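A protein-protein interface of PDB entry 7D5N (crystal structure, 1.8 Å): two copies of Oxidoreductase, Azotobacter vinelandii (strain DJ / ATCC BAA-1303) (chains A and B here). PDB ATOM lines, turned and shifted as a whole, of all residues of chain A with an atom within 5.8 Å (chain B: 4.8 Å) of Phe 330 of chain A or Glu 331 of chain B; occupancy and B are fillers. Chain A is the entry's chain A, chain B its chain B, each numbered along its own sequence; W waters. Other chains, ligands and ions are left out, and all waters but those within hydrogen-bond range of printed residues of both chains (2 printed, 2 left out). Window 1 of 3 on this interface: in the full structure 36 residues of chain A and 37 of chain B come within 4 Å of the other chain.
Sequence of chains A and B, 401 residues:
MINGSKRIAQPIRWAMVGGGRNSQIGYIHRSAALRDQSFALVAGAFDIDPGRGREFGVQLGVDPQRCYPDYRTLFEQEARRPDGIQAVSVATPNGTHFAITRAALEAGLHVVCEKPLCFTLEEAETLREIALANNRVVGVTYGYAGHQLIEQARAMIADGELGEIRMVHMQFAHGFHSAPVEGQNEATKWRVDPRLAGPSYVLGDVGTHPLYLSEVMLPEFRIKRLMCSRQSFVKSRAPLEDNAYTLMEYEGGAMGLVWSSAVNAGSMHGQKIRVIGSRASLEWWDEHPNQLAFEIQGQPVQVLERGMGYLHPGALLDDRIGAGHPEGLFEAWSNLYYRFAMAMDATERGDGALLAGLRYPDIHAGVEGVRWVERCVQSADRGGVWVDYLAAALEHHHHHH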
ATOM      1  N   TYR A  27      27.804 -19.953   4.731  1.00  0.00           N
ATOM      2  CA  TYR A  27      26.864 -19.457   5.755  1.00  0.00           C
ATOM      3  C   TYR A  27      25.645 -18.823   5.080  1.00  0.00           C
ATOM      4  O   TYR A  27      24.507 -19.074   5.537  1.00  0.00           O
ATOM      5  CB  TYR A  27      27.513 -18.496   6.748  1.00  0.00           C
ATOM      6  CG  TYR A  27      26.498 -17.935   7.704  1.00  0.00           C
ATOM      7  CD1 TYR A  27      25.830 -18.767   8.596  1.00  0.00           C
ATOM      8  CD2 TYR A  27      26.122 -16.602   7.658  1.00  0.00           C
ATOM      9  CE1 TYR A  27      24.845 -18.279   9.438  1.00  0.00           C
ATOM     10  CE2 TYR A  27      25.159 -16.096   8.518  1.00  0.00           C
ATOM     11  CZ  TYR A  27      24.526 -16.936   9.416  1.00  0.00           C
ATOM     12  OH  TYR A  27      23.562 -16.472  10.260  1.00  0.00           O
ATOM     13  N   ILE A  28      25.842 -18.036   4.029  1.00  0.00           N
ATOM     14  CA  ILE A  28      24.675 -17.311   3.453  1.00  0.00           C
ATOM     15  C   ILE A  28      23.698 -18.333   2.853  1.00  0.00           C
ATOM     16  O   ILE A  28      22.497 -18.075   2.914  1.00  0.00           O
ATOM     17  CB  ILE A  28      25.088 -16.195   2.473  1.00  0.00           C
ATOM     18  CG1 ILE A  28      23.858 -15.435   1.963  1.00  0.00           C
ATOM     19  CG2 ILE A  28      25.928 -16.715   1.327  1.00  0.00           C
ATOM     20  CD1 ILE A  28      24.193 -14.074   1.375  1.00  0.00           C
ATOM     21  N   SER A  31      21.776 -19.446   5.971  1.00  0.00           N
ATOM     22  CA  SER A  31      20.994 -18.316   6.527  1.00  0.00           C
ATOM     23  C   SER A  31      19.729 -18.114   5.662  1.00  0.00           C
ATOM     24  O   SER A  31      18.613 -17.930   6.211  1.00  0.00           O
ATOM     25  CB  SER A  31      21.862 -17.086   6.636  1.00  0.00           C
ATOM     26  OG  SER A  31      21.162 -16.008   7.229  1.00  0.00           O
ATOM     27  N   ALA A  32      19.878 -18.219   4.350  1.00  0.00           N
ATOM     28  CA  ALA A  32      18.768 -17.998   3.395  1.00  0.00           C
ATOM     29  C   ALA A  32      17.822 -19.216   3.339  1.00  0.00           C
ATOM     30  O   ALA A  32      16.599 -19.033   3.254  1.00  0.00           O
ATOM     31  CB  ALA A  32      19.337 -17.650   2.043  1.00  0.00           C
ATOM     32  N   ARG A  35      15.664 -19.891   6.565  1.00  0.00           N
ATOM     33  CA  ARG A  35      14.764 -18.770   6.916  1.00  0.00           C
ATOM     34  C   ARG A  35      13.327 -19.074   6.468  1.00  0.00           C
ATOM     35  O   ARG A  35      13.151 -19.717   5.427  1.00  0.00           O
ATOM     36  CB  ARG A  35      15.276 -17.504   6.248  1.00  0.00           C
ATOM     37  CG  ARG A  35      14.734 -16.217   6.844  1.00  0.00           C
ATOM     38  CD  ARG A  35      15.399 -15.091   6.081  1.00  0.00           C
ATOM     39  NE  ARG A  35      15.131 -13.792   6.666  1.00  0.00           N
ATOM     40  CZ  ARG A  35      15.685 -12.660   6.289  1.00  0.00           C
ATOM     41  NH1 ARG A  35      16.548 -12.646   5.291  1.00  0.00           N
ATOM     42  NH2 ARG A  35      15.346 -11.532   6.900  1.00  0.00           N
ATOM     43  N   GLY A 328      19.745  -6.222   3.041  1.00  0.00           N
ATOM     44  CA  GLY A 328      21.051  -6.528   2.456  1.00  0.00           C
ATOM     45  C   GLY A 328      21.025  -7.800   1.653  1.00  0.00           C
ATOM     46  O   GLY A 328      19.913  -8.293   1.299  1.00  0.00           O
ATOM     47  N   LEU A 329      22.212  -8.338   1.381  1.00  0.00           N
ATOM     48  CA  LEU A 329      22.339  -9.469   0.433  1.00  0.00           C
ATOM     49  C   LEU A 329      21.703 -10.731   1.035  1.00  0.00           C
ATOM     50  O   LEU A 329      21.249 -11.588   0.262  1.00  0.00           O
ATOM     51  CB  LEU A 329      23.815  -9.691   0.103  1.00  0.00           C
ATOM     52  CG  LEU A 329      24.089 -10.780  -0.924  1.00  0.00           C
ATOM     53  CD1 LEU A 329      23.368 -10.505  -2.225  1.00  0.00           C
ATOM     54  CD2 LEU A 329      25.581 -10.937  -1.154  1.00  0.00           C
ATOM     55  N   PHE A 330      21.640 -10.852   2.364  1.00  0.00           N
ATOM     56  CA  PHE A 330      20.971 -12.012   2.996  1.00  0.00           C
ATOM     57  C   PHE A 330      19.474 -12.007   2.648  1.00  0.00           C
ATOM     58  O   PHE A 330      18.899 -13.119   2.480  1.00  0.00           O
ATOM     59  CB  PHE A 330      21.212 -12.038   4.502  1.00  0.00           C
ATOM     60  CG  PHE A 330      22.598 -12.471   4.870  1.00  0.00           C
ATOM     61  CD1 PHE A 330      23.639 -11.552   4.945  1.00  0.00           C
ATOM     62  CD2 PHE A 330      22.872 -13.807   5.092  1.00  0.00           C
ATOM     63  CE1 PHE A 330      24.924 -11.964   5.263  1.00  0.00           C
ATOM     64  CE2 PHE A 330      24.155 -14.221   5.423  1.00  0.00           C
ATOM     65  CZ  PHE A 330      25.174 -13.296   5.524  1.00  0.00           C
ATOM     66  N   GLU A 331      18.861 -10.825   2.503  1.00  0.00           N
ATOM     67  CA  GLU A 331      17.426 -10.741   2.113  1.00  0.00           C
ATOM     68  C   GLU A 331      17.270 -11.196   0.661  1.00  0.00           C
ATOM     69  O   GLU A 331      16.334 -11.964   0.356  1.00  0.00           O
ATOM     70  CB  GLU A 331      16.829  -9.356   2.347  1.00  0.00           C
ATOM     71  CG  GLU A 331      16.461  -9.124   3.810  1.00  0.00           C
ATOM     72  CD  GLU A 331      17.653  -9.161   4.742  1.00  0.00           C
ATOM     73  OE1 GLU A 331      18.529  -8.279   4.561  1.00  0.00           O
ATOM     74  OE2 GLU A 331      17.724 -10.087   5.617  1.00  0.00           O
ATOM     75  N   ALA A 332      18.155 -10.741  -0.210  1.00  0.00           N
ATOM     76  CA  ALA A 332      18.146 -11.129  -1.632  1.00  0.00           C
ATOM     77  C   ALA A 332      18.253 -12.656  -1.735  1.00  0.00           C
ATOM     78  O   ALA A 332      17.478 -13.294  -2.502  1.00  0.00           O
ATOM     79  CB  ALA A 332      19.284 -10.443  -2.334  1.00  0.00           C
ATOM     80  N   TRP A 333      19.198 -13.253  -1.013  1.00  0.00           N
ATOM     81  CA  TRP A 333      19.402 -14.719  -1.092  1.00  0.00           C
ATOM     82  C   TRP A 333      18.177 -15.442  -0.545  1.00  0.00           C
ATOM     83  O   TRP A 333      17.831 -16.513  -1.075  1.00  0.00           O
ATOM     84  CB  TRP A 333      20.654 -15.122  -0.328  1.00  0.00           C
ATOM     85  CG  TRP A 333      21.905 -14.993  -1.130  1.00  0.00           C
ATOM     86  CD1 TRP A 333      22.442 -13.865  -1.686  1.00  0.00           C
ATOM     87  CD2 TRP A 333      22.798 -16.066  -1.454  1.00  0.00           C
ATOM     88  NE1 TRP A 333      23.616 -14.163  -2.325  1.00  0.00           N
ATOM     89  CE2 TRP A 333      23.862 -15.506  -2.196  1.00  0.00           C
ATOM     90  CE3 TRP A 333      22.801 -17.436  -1.173  1.00  0.00           C
ATOM     91  CZ2 TRP A 333      24.922 -16.281  -2.659  1.00  0.00           C
ATOM     92  CZ3 TRP A 333      23.840 -18.202  -1.641  1.00  0.00           C
ATOM     93  CH2 TRP A 333      24.886 -17.629  -2.374  1.00  0.00           C
ATOM     94  N   SER A 334      17.551 -14.887   0.485  1.00  0.00           N
ATOM     95  CA  SER A 334      16.350 -15.482   1.119  1.00  0.00           C
ATOM     96  C   SER A 334      15.211 -15.454   0.101  1.00  0.00           C
ATOM     97  O   SER A 334      14.392 -16.382   0.097  1.00  0.00           O
ATOM     98  CB  SER A 334      15.971 -14.781   2.382  1.00  0.00           C
ATOM     99  OG  SER A 334      17.033 -14.876   3.327  1.00  0.00           O
ATOM    100  N   ASN A 335      15.164 -14.403  -0.712  1.00  0.00           N
ATOM    101  CA  ASN A 335      14.125 -14.254  -1.754  1.00  0.00           C
ATOM    102  C   ASN A 335      14.337 -15.319  -2.838  1.00  0.00           C
ATOM    103  O   ASN A 335      13.327 -15.831  -3.344  1.00  0.00           O
ATOM    104  CB  ASN A 335      14.085 -12.829  -2.304  1.00  0.00           C
ATOM    105  CG  ASN A 335      13.688 -11.816  -1.250  1.00  0.00           C
ATOM    106  OD1 ASN A 335      12.977 -12.146  -0.307  1.00  0.00           O
ATOM    107  ND2 ASN A 335      14.105 -10.570  -1.426  1.00  0.00           N
ATOM    108  N   ARG B  35      17.432 -17.208  14.017  1.00  0.00           N
ATOM    109  CA  ARG B  35      18.673 -17.406  13.237  1.00  0.00           C
ATOM    110  C   ARG B  35      19.739 -18.096  14.096  1.00  0.00           C
ATOM    111  O   ARG B  35      19.830 -17.790  15.296  1.00  0.00           O
ATOM    112  CB  ARG B  35      19.150 -16.049  12.741  1.00  0.00           C
ATOM    113  CG  ARG B  35      20.116 -16.131  11.581  1.00  0.00           C
ATOM    114  CD  ARG B  35      20.455 -14.698  11.223  1.00  0.00           C
ATOM    115  NE  ARG B  35      21.222 -14.587  10.016  1.00  0.00           N
ATOM    116  CZ  ARG B  35      21.500 -13.437   9.415  1.00  0.00           C
ATOM    117  NH1 ARG B  35      21.085 -12.294   9.931  1.00  0.00           N
ATOM    118  NH2 ARG B  35      22.202 -13.441   8.306  1.00  0.00           N
ATOM    119  N   ARG B 320      29.233 -11.886   8.855  1.00  0.00           N
ATOM    120  CA  ARG B 320      28.548 -13.102   8.362  1.00  0.00           C
ATOM    121  C   ARG B 320      28.911 -13.365   6.901  1.00  0.00           C
ATOM    122  O   ARG B 320      28.622 -14.452   6.411  1.00  0.00           O
ATOM    123  CB  ARG B 320      27.049 -12.922   8.570  1.00  0.00           C
ATOM    124  CG  ARG B 320      26.630 -13.003  10.022  1.00  0.00           C
ATOM    125  CD  ARG B 320      25.300 -12.305  10.219  1.00  0.00           C
ATOM    126  NE  ARG B 320      24.976 -12.103  11.619  1.00  0.00           N
ATOM    127  CZ  ARG B 320      24.419 -13.001  12.427  1.00  0.00           C
ATOM    128  NH1 ARG B 320      24.103 -14.204  11.987  1.00  0.00           N
ATOM    129  NH2 ARG B 320      24.173 -12.679  13.681  1.00  0.00           N
ATOM    130  N   ILE B 321      29.604 -12.428   6.251  1.00  0.00           N
ATOM    131  CA  ILE B 321      30.004 -12.552   4.831  1.00  0.00           C
ATOM    132  C   ILE B 321      31.120 -11.531   4.613  1.00  0.00           C
ATOM    133  O   ILE B 321      31.169 -10.553   5.366  1.00  0.00           O
ATOM    134  CB  ILE B 321      28.811 -12.345   3.878  1.00  0.00           C
ATOM    135  CG1 ILE B 321      29.194 -12.780   2.456  1.00  0.00           C
ATOM    136  CG2 ILE B 321      28.304 -10.908   3.950  1.00  0.00           C
ATOM    137  CD1 ILE B 321      28.024 -12.957   1.534  1.00  0.00           C
ATOM    138  N   PRO B 326      26.838  -6.265   1.076  1.00  0.00           N
ATOM    139  CA  PRO B 326      26.109  -5.480   2.064  1.00  0.00           C
ATOM    140  C   PRO B 326      25.339  -6.358   3.063  1.00  0.00           C
ATOM    141  O   PRO B 326      24.481  -7.139   2.672  1.00  0.00           O
ATOM    142  CB  PRO B 326      25.122  -4.659   1.232  1.00  0.00           C
ATOM    143  CG  PRO B 326      24.903  -5.496  -0.002  1.00  0.00           C
ATOM    144  CD  PRO B 326      26.198  -6.253  -0.253  1.00  0.00           C
ATOM    145  N   GLU B 327      25.664  -6.213   4.344  1.00  0.00           N
ATOM    146  CA  GLU B 327      24.779  -6.648   5.438  1.00  0.00           C
ATOM    147  C   GLU B 327      23.724  -5.562   5.615  1.00  0.00           C
ATOM    148  O   GLU B 327      23.859  -4.455   5.023  1.00  0.00           O
ATOM    149  CB  GLU B 327      25.589  -6.925   6.705  1.00  0.00           C
ATOM    150  CG  GLU B 327      26.469  -8.150   6.549  1.00  0.00           C
ATOM    151  CD  GLU B 327      27.119  -8.723   7.795  1.00  0.00           C
ATOM    152  OE1 GLU B 327      26.873  -8.206   8.891  1.00  0.00           O
ATOM    153  OE2 GLU B 327      27.852  -9.718   7.645  1.00  0.00           O
ATOM    154  N   GLY B 328      22.698  -5.858   6.391  1.00  0.00           N
ATOM    155  CA  GLY B 328      21.607  -4.910   6.636  1.00  0.00           C
ATOM    156  C   GLY B 328      21.103  -4.988   8.061  1.00  0.00           C
ATOM    157  O   GLY B 328      21.803  -5.579   8.955  1.00  0.00           O
ATOM    158  N   LEU B 329      19.955  -4.367   8.310  1.00  0.00           N
ATOM    159  CA  LEU B 329      19.458  -4.209   9.704  1.00  0.00           C
ATOM    160  C   LEU B 329      19.127  -5.588  10.293  1.00  0.00           C
ATOM    161  O   LEU B 329      19.158  -5.737  11.526  1.00  0.00           O
ATOM    162  CB  LEU B 329      18.245  -3.276   9.725  1.00  0.00           C
ATOM    163  CG  LEU B 329      17.631  -3.041  11.097  1.00  0.00           C
ATOM    164  CD1 LEU B 329      18.645  -2.394  12.052  1.00  0.00           C
ATOM    165  CD2 LEU B 329      16.390  -2.190  10.991  1.00  0.00           C
ATOM    166  N   PHE B 330      18.792  -6.574   9.466  1.00  0.00           N
ATOM    167  CA  PHE B 330      18.504  -7.944   9.963  1.00  0.00           C
ATOM    168  C   PHE B 330      19.762  -8.545  10.585  1.00  0.00           C
ATOM    169  O   PHE B 330      19.608  -9.265  11.594  1.00  0.00           O
ATOM    170  CB  PHE B 330      17.932  -8.863   8.884  1.00  0.00           C
ATOM    171  CG  PHE B 330      16.508  -8.533   8.543  1.00  0.00           C
ATOM    172  CD1 PHE B 330      16.231  -7.553   7.607  1.00  0.00           C
ATOM    173  CD2 PHE B 330      15.449  -9.152   9.197  1.00  0.00           C
ATOM    174  CE1 PHE B 330      14.920  -7.236   7.288  1.00  0.00           C
ATOM    175  CE2 PHE B 330      14.134  -8.843   8.872  1.00  0.00           C
ATOM    176  CZ  PHE B 330      13.877  -7.874   7.927  1.00  0.00           C
ATOM    177  N   GLU B 331      20.946  -8.259  10.034  1.00  0.00           N
ATOM    178  CA  GLU B 331      22.208  -8.761  10.636  1.00  0.00           C
ATOM    179  C   GLU B 331      22.405  -8.078  11.998  1.00  0.00           C
ATOM    180  O   GLU B 331      22.798  -8.774  12.982  1.00  0.00           O
ATOM    181  CB  GLU B 331      23.394  -8.544   9.691  1.00  0.00           C
ATOM    182  CG  GLU B 331      23.461  -9.574   8.572  1.00  0.00           C
ATOM    183  CD  GLU B 331      22.252  -9.551   7.649  1.00  0.00           C
ATOM    184  OE1 GLU B 331      21.483 -10.544   7.637  1.00  0.00           O
ATOM    185  OE2 GLU B 331      22.033  -8.491   7.022  1.00  0.00           O
ATOM    186  N   ALA B 332      22.145  -6.769  12.079  1.00  0.00           N
ATOM    187  CA  ALA B 332      22.293  -5.993  13.336  1.00  0.00           C
ATOM    188  C   ALA B 332      21.389  -6.609  14.413  1.00  0.00           C
ATOM    189  O   ALA B 332      21.832  -6.827  15.544  1.00  0.00           O
ATOM    190  CB  ALA B 332      21.965  -4.539  13.120  1.00  0.00           C
ATOM    191  N   TRP B 333      20.148  -6.924  14.062  1.00  0.00           N
ATOM    192  CA  TRP B 333      19.190  -7.486  15.042  1.00  0.00           C
ATOM    193  C   TRP B 333      19.632  -8.891  15.450  1.00  0.00           C
ATOM    194  O   TRP B 333      19.487  -9.223  16.642  1.00  0.00           O
ATOM    195  CB  TRP B 333      17.768  -7.497  14.478  1.00  0.00           C
ATOM    196  CG  TRP B 333      17.034  -6.212  14.632  1.00  0.00           C
ATOM    197  CD1 TRP B 333      17.373  -4.989  14.125  1.00  0.00           C
ATOM    198  CD2 TRP B 333      15.828  -6.021  15.374  1.00  0.00           C
ATOM    199  NE1 TRP B 333      16.451  -4.056  14.497  1.00  0.00           N
ATOM    200  CE2 TRP B 333      15.488  -4.658  15.261  1.00  0.00           C
ATOM    201  CE3 TRP B 333      14.992  -6.874  16.098  1.00  0.00           C
ATOM    202  CZ2 TRP B 333      14.331  -4.134  15.830  1.00  0.00           C
ATOM    203  CZ3 TRP B 333      13.879  -6.347  16.705  1.00  0.00           C
ATOM    204  CH2 TRP B 333      13.548  -4.995  16.567  1.00  0.00           C
ATOM    205  N   SER B 334      20.155  -9.685  14.509  1.00  0.00           N
ATOM    206  CA  SER B 334      20.671 -11.052  14.759  1.00  0.00           C
ATOM    207  C   SER B 334      21.853 -10.966  15.739  1.00  0.00           C
ATOM    208  O   SER B 334      22.041 -11.885  16.595  1.00  0.00           O
ATOM    209  CB  SER B 334      21.050 -11.759  13.463  1.00  0.00           C
ATOM    210  OG  SER B 334      19.931 -11.841  12.566  1.00  0.00           O
ATOM    211  N   ASN B 335      22.674  -9.929  15.595  1.00  0.00           N
ATOM    212  CA  ASN B 335      23.848  -9.722  16.481  1.00  0.00           C
ATOM    213  C   ASN B 335      23.372  -9.419  17.908  1.00  0.00           C
ATOM    214  O   ASN B 335      24.056  -9.878  18.849  1.00  0.00           O
ATOM    215  CB  ASN B 335      24.789  -8.657  15.916  1.00  0.00           C
ATOM    216  CG  ASN B 335      25.406  -9.095  14.607  1.00  0.00           C
ATOM    217  OD1 ASN B 335      25.554 -10.285  14.346  1.00  0.00           O
ATOM    218  ND2 ASN B 335      25.805  -8.144  13.781  1.00  0.00           N
HETATM  219  O   HOH W   1      28.625 -16.449   3.963  1.00  0.00           O
HETATM  220  O   HOH W   2      19.046 -11.646   7.258  1.00  0.00           O
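Arg 35 of chain A touches Phe 330 of chain B, and with the chains exchanged Phe 330 of chain A touches Arg 35 of chain B. Phe 330 of chain A touches Glu 331 of chain B, and with the chains exchanged Glu 331 of chain A touches Phe 330 of chain B. 9 positions are printed for both chains.
The backbone NH (N) of Gly 328 of chain A lies within hydrogen-bond range of the side-chain carboxylate (OE1) of Glu 331 of chain A, at 2.8 Å. The backbone carbonyl oxygen (O) of Phe 330 of chain A lies within hydrogen-bond range of the side-chain hydroxyl (OG) of Ser 334 of chain A, 2.7 Å away. N of Arg 320 of chain B lies within hydrogen-bond range of OE2 of Glu 327 of chain B, at 2.8 Å. OD1 of Asn 335 of chain B is in hydrogen-bond range of NH2 of Arg 320 of chain B. N of Gly 328 of chain B is in hydrogen-bond range of OE2 of Glu 331 of chain B (2.8 Å). O of Phe 330 of chain B is in hydrogen-bond range of OG of Ser 334 of chain B (2.8 Å).
OH of Tyr 27 of chain A sits at hydrogen-bond distance from NE of Arg 35 of chain B (3.0 Å). OH of Tyr 27 of chain A lies within hydrogen-bond range of NH1 of Arg 320 of chain B (2.9 Å). OG of Ser 31 of chain A lies within hydrogen-bond range of NH2 of Arg 35 of chain B. The backbone NH of Leu 329 of chain A lies within hydrogen-bond range of the backbone carbonyl oxygen of Pro 326 of chain B (2.9 Å).
Water W2 lies within hydrogen-bond range of OE2 of Glu 331 of chain A (2.6 Å), OE1 of Glu 331 of chain B (2.7 Å), NH1 of Arg 35 of chain A (3.3 Å) and NH1 of Arg 35 of chain B (3.4 Å). Water W1 lies within hydrogen-bond range of O of Arg 320 of chain B (3.2 Å) and N of Ile 28 of chain A (3.2 Å).
Among the printed residues, merely in contact across the chains: Phe 330 of chain A with Arg 35 of chain B (3.3 Å), Arg 35 of chain A with Phe 330 of chain B (3.3 Å), Phe 330 of chain A with Glu 331 of chain B (3.5 Å), Gly 328 of chain A with Pro 326 of chain B (3.5 Å), Glu 331 of chain A with Phe 330 of chain B (3.5 Å), Phe 330 of chain A with Arg 320 of chain B (3.6 Å), Phe 330 of chain A with Ile 321 of chain B (3.8 Å) and Ile 28 of chain A with Ile 321 of chain B (3.99 Å).
Hydrophobic or aromatic side chains of chain A that line the printed part of chain B: Tyr 27, Ile 28, Leu 329 and Phe 330. Of the 13 printed residues of chain B, 6 touch a printed residue of chain A. Among the printed residues, 12 pairs touch across the chains. Among the printed residues, no Asp or Glu carboxylate lies within 4 Å of a Lys or Arg side-chain nitrogen of the other chain.
Of chain B, only Arg 35 (3.3 Å), Arg 320 (3.6 Å), Ile 321 (3.8 Å) and Glu 331 (3.5 Å) come within 4 Å of Phe 330 of chain A. Of chain A, only Phe 330 comes within 4 Å of Glu 331 of chain B. Of the printed residues of chain B, Arg 35 of chain A touches Phe 330 (3.3 Å). Of the printed residues of chain A, Ile 321 of chain B touches Ile 28 and Phe 330. Of the printed residues of chain A, Arg 320 of chain B touches Tyr 27 (2.9 Å) and Phe 330 (3.6 Å). Of the printed residues of chain B, Leu 329 of chain A touches Pro 326. The nearest residue of chain B that does not touch Phe 330 of chain A is Glu 327 of chain B (4.3 Å). The nearest printed residue of chain B that does not touch Leu 329 of chain A is Ile 321 of chain B (4.2 Å).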
